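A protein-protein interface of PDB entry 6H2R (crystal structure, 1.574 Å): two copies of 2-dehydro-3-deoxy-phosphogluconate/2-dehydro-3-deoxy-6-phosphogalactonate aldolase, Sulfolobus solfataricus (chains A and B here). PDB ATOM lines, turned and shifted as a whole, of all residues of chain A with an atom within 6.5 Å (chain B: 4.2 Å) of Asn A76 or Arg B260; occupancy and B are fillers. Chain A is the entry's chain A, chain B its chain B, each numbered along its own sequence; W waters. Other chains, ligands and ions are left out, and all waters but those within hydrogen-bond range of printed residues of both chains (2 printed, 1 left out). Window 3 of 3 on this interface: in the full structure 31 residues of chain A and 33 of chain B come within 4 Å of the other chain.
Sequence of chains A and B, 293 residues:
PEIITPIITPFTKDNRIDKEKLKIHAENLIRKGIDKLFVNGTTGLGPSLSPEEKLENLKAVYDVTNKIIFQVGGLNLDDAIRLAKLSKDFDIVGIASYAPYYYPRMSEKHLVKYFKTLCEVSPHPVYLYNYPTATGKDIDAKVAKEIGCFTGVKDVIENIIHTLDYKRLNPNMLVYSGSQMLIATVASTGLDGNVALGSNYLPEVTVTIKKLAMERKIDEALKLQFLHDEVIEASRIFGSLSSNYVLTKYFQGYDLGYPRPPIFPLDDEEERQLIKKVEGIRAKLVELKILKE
The backbone NH (N) of Gly A74 is in hydrogen-bond range of the side-chain hydroxyl (OH) of Tyr A114, at 3.4 Å.
N of Asp A78 sits at hydrogen-bond distance from OD1 of Asn A76.
The backbone NH of Asp A79 is in hydrogen-bond range of the side-chain amide oxygen of Asn A76 (3.4 Å).
The side-chain amide oxygen of Asn B15 lies within hydrogen-bond range of the guanidinium group of Arg B260 (2.8 Å).
O of Ser B48 lies within hydrogen-bond range of NH1 of Arg B260 (2.9 Å).
The guanidinium group (NH1) of Arg B260 is in salt-bridge range of the side-chain carboxylate (OE1) of Glu B53, 2.8 Å away.
Among the printed residues, pairs that only touch across the chains: Leu A75 with Pro B262 (3.4 Å), Leu A75 with Ser B48 (3.6 Å), Leu A75 with Pro B261 (3.6 Å), Tyr A114 with Pro B262 (3.7 Å) and Asn A76 with Pro B261 (3.9 Å).
OD1 of Asn A76 lies within hydrogen-bond range of ND2 of Asn B15.
The side-chain amide nitrogen (ND2) of Asn A76 sits close to the guanidinium group (NH1) of Arg B260 (3.5 Å).
The backbone NH (N) of Leu A77 sits at hydrogen-bond distance from the backbone carbonyl oxygen (O) of Pro B261 (3.0 Å).
The side-chain carboxylate (OD2) of Asp A78 sits at hydrogen-bond distance from the side-chain amide nitrogen (ND2) of Asn B15, at 3.0 Å.
Water W2 lies within hydrogen-bond range of OG of Ser B48 (2.6 Å), O of Leu A75 (2.7 Å) and O of Arg B260 (2.9 Å).
Water W1 lies within hydrogen-bond range of the side-chain amide nitrogen (ND2) of Asn A76 (2.9 Å), the side-chain carboxylate (OE1) of Glu B53 (3.0 Å) and the guanidinium group (NH1) of Arg B260 (3.3 Å).
Of the 11 printed residues of chain B, 5 touch a printed residue of chain A.
Hydrophobic or aromatic side chains of chain B that line the printed part of chain A: Pro B262.
Printed residues of chain A that touch a printed residue of chain B: Leu A75, Asn A76, Leu A77, Asp A78 and Tyr A114.
Hydrophobic or aromatic side chains of chain A that line the printed part of chain B: Leu A75, Leu A77 and Tyr A114.
No position is printed for both chains.
Of the 9 pairs that touch across the chains among the printed residues, none has its exchanged pair printed and touching as well.
Asn A76 touches three residues of chain B.
Of the printed residues of chain A, Arg B260 touches Asn A76 (3.5 Å).
Of the printed residues of chain A, Asn B15 touches Asn A76 and Asp A78.
Printed residues of chain B within 4 Å of Tyr A114: Pro B262.
Of the printed residues of chain A, Ser B48 touches Leu A75.
Gly A73 touches none of the printed residues of chain B.
The nearest printed residue of chain B that does not touch Asn A76 is Ser B48 (4.3 Å).
The nearest residue of chain A that does not touch Arg B260 is Leu A75 (4.1 Å).
The nearest printed residue of chain B that does not touch Asp A78 is Pro B261 (5.0 Å).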
ATOM      1  N   VAL A  72      -1.874  34.585  24.745  1.00  0.00           N
ATOM      2  CA  VAL A  72      -1.790  33.509  23.762  1.00  0.00           C
ATOM      3  C   VAL A  72      -1.735  32.127  24.371  1.00  0.00           C
ATOM      4  O   VAL A  72      -1.661  31.146  23.617  1.00  0.00           O
ATOM      5  CB  VAL A  72      -0.568  33.661  22.834  1.00  0.00           C
ATOM      6  CG1 VAL A  72      -0.642  34.986  22.053  1.00  0.00           C
ATOM      7  CG2 VAL A  72       0.703  33.511  23.565  1.00  0.00           C
ATOM      8  N   GLY A  73      -1.729  32.007  25.692  1.00  0.00           N
ATOM      9  CA  GLY A  73      -1.437  30.751  26.362  1.00  0.00           C
ATOM     10  C   GLY A  73      -2.527  29.718  26.252  1.00  0.00           C
ATOM     11  O   GLY A  73      -3.685  29.981  25.951  1.00  0.00           O
ATOM     12  N   GLY A  74      -2.130  28.493  26.566  1.00  0.00           N
ATOM     13  CA  GLY A  74      -3.075  27.398  26.594  1.00  0.00           C
ATOM     14  C   GLY A  74      -2.377  26.087  26.904  1.00  0.00           C
ATOM     15  O   GLY A  74      -1.184  26.049  27.181  1.00  0.00           O
ATOM     16  N   LEU A  75      -3.138  25.006  26.765  1.00  0.00           N
ATOM     17  CA  LEU A  75      -2.643  23.679  27.102  1.00  0.00           C
ATOM     18  C   LEU A  75      -2.088  22.910  25.897  1.00  0.00           C
ATOM     19  O   LEU A  75      -1.710  21.736  26.027  1.00  0.00           O
ATOM     20  CB  LEU A  75      -3.735  22.879  27.796  1.00  0.00           C
ATOM     21  CG  LEU A  75      -4.080  23.438  29.192  1.00  0.00           C
ATOM     22  CD1 LEU A  75      -5.212  22.602  29.801  1.00  0.00           C
ATOM     23  CD2 LEU A  75      -2.846  23.456  30.077  1.00  0.00           C
ATOM     24  N   ASN A  76      -2.019  23.533  24.725  1.00  0.00           N
ATOM     25  CA  ASN A  76      -1.340  22.988  23.551  1.00  0.00           C
ATOM     26  C   ASN A  76      -0.252  23.993  23.206  1.00  0.00           C
ATOM     27  O   ASN A  76      -0.517  25.057  22.625  1.00  0.00           O
ATOM     28  CB  ASN A  76      -2.317  22.759  22.411  1.00  0.00           C
ATOM     29  CG  ASN A  76      -1.649  22.169  21.195  1.00  0.00           C
ATOM     30  OD1 ASN A  76      -0.458  22.339  20.998  1.00  0.00           O
ATOM     31  ND2 ASN A  76      -2.419  21.496  20.371  1.00  0.00           N
ATOM     32  N   LEU A  77       0.986  23.696  23.606  1.00  0.00           N
ATOM     33  CA  LEU A  77       2.067  24.662  23.414  1.00  0.00           C
ATOM     34  C   LEU A  77       2.273  24.985  21.941  1.00  0.00           C
ATOM     35  O   LEU A  77       2.585  26.146  21.599  1.00  0.00           O
ATOM     36  CB  LEU A  77       3.347  24.130  24.036  1.00  0.00           C
ATOM     37  CG  LEU A  77       4.620  24.976  23.924  1.00  0.00           C
ATOM     38  CD1 LEU A  77       4.390  26.411  24.367  1.00  0.00           C
ATOM     39  CD2 LEU A  77       5.725  24.321  24.735  1.00  0.00           C
ATOM     40  N   ASP A  78       2.005  24.027  21.042  1.00  0.00           N
ATOM     41  CA  ASP A  78       2.138  24.337  19.618  1.00  0.00           C
ATOM     42  C   ASP A  78       1.183  25.457  19.205  1.00  0.00           C
ATOM     43  O   ASP A  78       1.518  26.293  18.354  1.00  0.00           O
ATOM     44  CB  ASP A  78       1.887  23.099  18.764  1.00  0.00           C
ATOM     45  CG  ASP A  78       3.083  22.169  18.736  1.00  0.00           C
ATOM     46  OD1 ASP A  78       4.158  22.547  19.264  1.00  0.00           O
ATOM     47  OD2 ASP A  78       2.917  21.057  18.167  1.00  0.00           O
ATOM     48  N   ASP A  79      -0.030  25.474  19.765  1.00  0.00           N
ATOM     49  CA  ASP A  79      -0.973  26.534  19.387  1.00  0.00           C
ATOM     50  C   ASP A  79      -0.527  27.884  19.947  1.00  0.00           C
ATOM     51  O   ASP A  79      -0.707  28.931  19.302  1.00  0.00           O
ATOM     52  CB  ASP A  79      -2.385  26.199  19.882  1.00  0.00           C
ATOM     53  CG  ASP A  79      -3.127  25.231  18.969  1.00  0.00           C
ATOM     54  OD1 ASP A  79      -2.763  25.128  17.785  1.00  0.00           O
ATOM     55  OD2 ASP A  79      -4.070  24.606  19.454  1.00  0.00           O
ATOM     56  N   ALA A  80      -0.003  27.898  21.183  1.00  0.00           N
ATOM     57  CA  ALA A  80       0.539  29.132  21.738  1.00  0.00           C
ATOM     58  C   ALA A  80       1.710  29.660  20.897  1.00  0.00           C
ATOM     59  O   ALA A  80       1.812  30.870  20.637  1.00  0.00           O
ATOM     60  CB  ALA A  80       0.960  28.896  23.184  1.00  0.00           C
ATOM     61  N   ILE A  81       2.571  28.761  20.437  1.00  0.00           N
ATOM     62  CA  ILE A  81       3.656  29.139  19.525  1.00  0.00           C
ATOM     63  C   ILE A  81       3.102  29.734  18.240  1.00  0.00           C
ATOM     64  O   ILE A  81       3.576  30.779  17.774  1.00  0.00           O
ATOM     65  CB  ILE A  81       4.566  27.923  19.266  1.00  0.00           C
ATOM     66  CG1 ILE A  81       5.343  27.558  20.531  1.00  0.00           C
ATOM     67  CG2 ILE A  81       5.445  28.196  18.052  1.00  0.00           C
ATOM     68  CD1 ILE A  81       6.076  26.240  20.406  1.00  0.00           C
ATOM     69  N   ARG A  82       2.080  29.107  17.661  1.00  0.00           N
ATOM     70  CA  ARG A  82       1.517  29.606  16.405  1.00  0.00           C
ATOM     71  C   ARG A  82       0.886  30.992  16.573  1.00  0.00           C
ATOM     72  O   ARG A  82       0.932  31.817  15.650  1.00  0.00           O
ATOM     73  CB  ARG A  82       0.489  28.625  15.853  1.00  0.00           C
ATOM     74  CG  ARG A  82       1.076  27.439  15.089  1.00  0.00           C
ATOM     75  CD  ARG A  82      -0.018  26.555  14.437  1.00  0.00           C
ATOM     76  NE  ARG A  82      -0.682  25.673  15.404  1.00  0.00           N
ATOM     77  CZ  ARG A  82      -0.386  24.388  15.592  1.00  0.00           C
ATOM     78  NH1 ARG A  82       0.556  23.795  14.892  1.00  0.00           N
ATOM     79  NH2 ARG A  82      -1.030  23.700  16.502  1.00  0.00           N
ATOM     80  N   TYR A 114       7.913  25.717  29.531  1.00  0.00           N
ATOM     81  CA  TYR A 114       6.789  26.303  28.811  1.00  0.00           C
ATOM     82  C   TYR A 114       7.052  27.770  28.491  1.00  0.00           C
ATOM     83  O   TYR A 114       6.909  28.205  27.342  1.00  0.00           O
ATOM     84  CB  TYR A 114       5.511  26.148  29.640  1.00  0.00           C
ATOM     85  CG  TYR A 114       4.302  26.883  29.098  1.00  0.00           C
ATOM     86  CD1 TYR A 114       3.546  26.343  28.051  1.00  0.00           C
ATOM     87  CD2 TYR A 114       3.955  28.148  29.555  1.00  0.00           C
ATOM     88  CE1 TYR A 114       2.444  27.026  27.536  1.00  0.00           C
ATOM     89  CE2 TYR A 114       2.894  28.828  29.044  1.00  0.00           C
ATOM     90  CZ  TYR A 114       2.124  28.278  28.037  1.00  0.00           C
ATOM     91  OH  TYR A 114       1.049  28.970  27.512  1.00  0.00           O
ATOM     92  N   PHE B  11       0.658  10.569  21.746  1.00  0.00           N
ATOM     93  CA  PHE B  11       0.963  11.532  20.696  1.00  0.00           C
ATOM     94  C   PHE B  11       2.235  11.150  19.954  1.00  0.00           C
ATOM     95  O   PHE B  11       3.149  10.536  20.514  1.00  0.00           O
ATOM     96  CB  PHE B  11       1.118  12.948  21.261  1.00  0.00           C
ATOM     97  CG  PHE B  11      -0.110  13.463  21.941  1.00  0.00           C
ATOM     98  CD1 PHE B  11      -0.323  13.195  23.288  1.00  0.00           C
ATOM     99  CD2 PHE B  11      -1.053  14.202  21.249  1.00  0.00           C
ATOM    100  CE1 PHE B  11      -1.442  13.648  23.939  1.00  0.00           C
ATOM    101  CE2 PHE B  11      -2.211  14.665  21.912  1.00  0.00           C
ATOM    102  CZ  PHE B  11      -2.383  14.382  23.248  1.00  0.00           C
ATOM    103  N   ASN B  15       3.258  15.793  17.708  1.00  0.00           N
ATOM    104  CA  ASN B  15       2.140  16.275  18.533  1.00  0.00           C
ATOM    105  C   ASN B  15       0.776  16.008  17.903  1.00  0.00           C
ATOM    106  O   ASN B  15      -0.152  16.804  18.034  1.00  0.00           O
ATOM    107  CB  ASN B  15       2.319  17.762  18.841  1.00  0.00           C
ATOM    108  CG  ASN B  15       1.402  18.242  19.924  1.00  0.00           C
ATOM    109  OD1 ASN B  15       1.037  17.485  20.842  1.00  0.00           O
ATOM    110  ND2 ASN B  15       1.041  19.503  19.843  1.00  0.00           N
ATOM    111  N   LEU B  45      -5.115  13.591  29.016  1.00  0.00           N
ATOM    112  CA  LEU B  45      -4.878  15.002  28.662  1.00  0.00           C
ATOM    113  C   LEU B  45      -6.085  15.633  27.968  1.00  0.00           C
ATOM    114  O   LEU B  45      -5.947  16.467  27.052  1.00  0.00           O
ATOM    115  CB  LEU B  45      -3.613  15.177  27.823  1.00  0.00           C
ATOM    116  CG  LEU B  45      -2.340  14.580  28.391  1.00  0.00           C
ATOM    117  CD1 LEU B  45      -1.084  15.029  27.659  1.00  0.00           C
ATOM    118  CD2 LEU B  45      -2.194  14.855  29.877  1.00  0.00           C
ATOM    119  N   SER B  48      -6.213  19.252  27.104  1.00  0.00           N
ATOM    120  CA  SER B  48      -5.224  19.628  26.107  1.00  0.00           C
ATOM    121  C   SER B  48      -5.669  19.301  24.686  1.00  0.00           C
ATOM    122  O   SER B  48      -4.952  19.648  23.734  1.00  0.00           O
ATOM    123  CB  SER B  48      -3.896  18.925  26.390  1.00  0.00           C
ATOM    124  OG  SER B  48      -3.495  19.107  27.719  1.00  0.00           O
ATOM    125  N   LEU B  49      -6.790  18.619  24.546  1.00  0.00           N
ATOM    126  CA  LEU B  49      -7.341  18.209  23.263  1.00  0.00           C
ATOM    127  C   LEU B  49      -8.443  19.151  22.786  1.00  0.00           C
ATOM    128  O   LEU B  49      -9.325  19.563  23.561  1.00  0.00           O
ATOM    129  CB  LEU B  49      -7.952  16.808  23.369  1.00  0.00           C
ATOM    130  CG  LEU B  49      -7.003  15.711  23.864  1.00  0.00           C
ATOM    131  CD1 LEU B  49      -7.754  14.381  24.064  1.00  0.00           C
ATOM    132  CD2 LEU B  49      -5.884  15.516  22.871  1.00  0.00           C
ATOM    133  N   GLU B  53     -10.162  16.658  18.346  1.00  0.00           N
ATOM    134  CA  GLU B  53      -9.322  15.574  18.819  1.00  0.00           C
ATOM    135  C   GLU B  53     -10.030  14.697  19.850  1.00  0.00           C
ATOM    136  O   GLU B  53      -9.787  13.481  19.887  1.00  0.00           O
ATOM    137  CB  GLU B  53      -8.033  16.143  19.414  1.00  0.00           C
ATOM    138  CG  GLU B  53      -7.075  16.755  18.351  1.00  0.00           C
ATOM    139  CD  GLU B  53      -5.951  17.572  18.943  1.00  0.00           C
ATOM    140  OE1 GLU B  53      -6.144  18.287  19.983  1.00  0.00           O
ATOM    141  OE2 GLU B  53      -4.843  17.535  18.344  1.00  0.00           O
ATOM    142  N   PRO B 259       3.693  12.598  25.575  1.00  0.00           N
ATOM    143  CA  PRO B 259       2.613  13.507  26.008  1.00  0.00           C
ATOM    144  C   PRO B 259       2.600  14.759  25.154  1.00  0.00           C
ATOM    145  O   PRO B 259       3.450  14.937  24.270  1.00  0.00           O
ATOM    146  CB  PRO B 259       2.949  13.792  27.476  1.00  0.00           C
ATOM    147  CG  PRO B 259       4.398  13.540  27.608  1.00  0.00           C
ATOM    148  CD  PRO B 259       4.834  12.612  26.493  1.00  0.00           C
ATOM    149  N   ARG B 260       1.647  15.644  25.418  1.00  0.00           N
ATOM    150  CA  ARG B 260       1.530  16.904  24.709  1.00  0.00           C
ATOM    151  C   ARG B 260       2.060  18.036  25.577  1.00  0.00           C
ATOM    152  O   ARG B 260       1.453  18.326  26.629  1.00  0.00           O
ATOM    153  CB  ARG B 260       0.080  17.160  24.337  1.00  0.00           C
ATOM    154  CG  ARG B 260      -0.183  18.598  23.902  1.00  0.00           C
ATOM    155  CD  ARG B 260      -1.534  18.727  23.186  1.00  0.00           C
ATOM    156  NE  ARG B 260      -1.482  18.181  21.828  1.00  0.00           N
ATOM    157  CZ  ARG B 260      -2.526  18.083  21.027  1.00  0.00           C
ATOM    158  NH1 ARG B 260      -3.723  18.457  21.438  1.00  0.00           N
ATOM    159  NH2 ARG B 260      -2.382  17.616  19.804  1.00  0.00           N
ATOM    160  N   PRO B 261       3.136  18.731  25.172  1.00  0.00           N
ATOM    161  CA  PRO B 261       3.618  19.900  25.941  1.00  0.00           C
ATOM    162  C   PRO B 261       2.514  20.939  26.113  1.00  0.00           C
ATOM    163  O   PRO B 261       1.756  21.208  25.173  1.00  0.00           O
ATOM    164  CB  PRO B 261       4.767  20.438  25.067  1.00  0.00           C
ATOM    165  CG  PRO B 261       5.282  19.231  24.385  1.00  0.00           C
ATOM    166  CD  PRO B 261       4.060  18.391  24.070  1.00  0.00           C
ATOM    167  N   PRO B 262       2.395  21.559  27.297  1.00  0.00           N
ATOM    168  CA  PRO B 262       3.347  21.602  28.408  1.00  0.00           C
ATOM    169  C   PRO B 262       3.405  20.400  29.366  1.00  0.00           C
ATOM    170  O   PRO B 262       4.092  20.476  30.378  1.00  0.00           O
ATOM    171  CB  PRO B 262       2.885  22.850  29.208  1.00  0.00           C
ATOM    172  CG  PRO B 262       1.454  22.871  28.967  1.00  0.00           C
ATOM    173  CD  PRO B 262       1.285  22.507  27.512  1.00  0.00           C
ATOM    174  N   ILE B 263       2.748  19.301  29.031  1.00  0.00           N
ATOM    175  CA  ILE B 263       3.039  18.018  29.654  1.00  0.00           C
ATOM    176  C   ILE B 263       4.238  17.457  28.887  1.00  0.00           C
ATOM    177  O   ILE B 263       4.071  16.760  27.895  1.00  0.00           O
ATOM    178  CB  ILE B 263       1.835  17.058  29.617  1.00  0.00           C
ATOM    179  CG1 ILE B 263       0.593  17.731  30.232  1.00  0.00           C
ATOM    180  CG2 ILE B 263       2.175  15.780  30.357  1.00  0.00           C
ATOM    181  CD1 ILE B 263       0.778  18.241  31.649  1.00  0.00           C
HETATM  182  O   HOH W   1      -5.317  21.116  20.345  1.00  0.00           O
HETATM  183  O   HOH W   2      -0.924  19.653  27.580  1.00  0.00           O
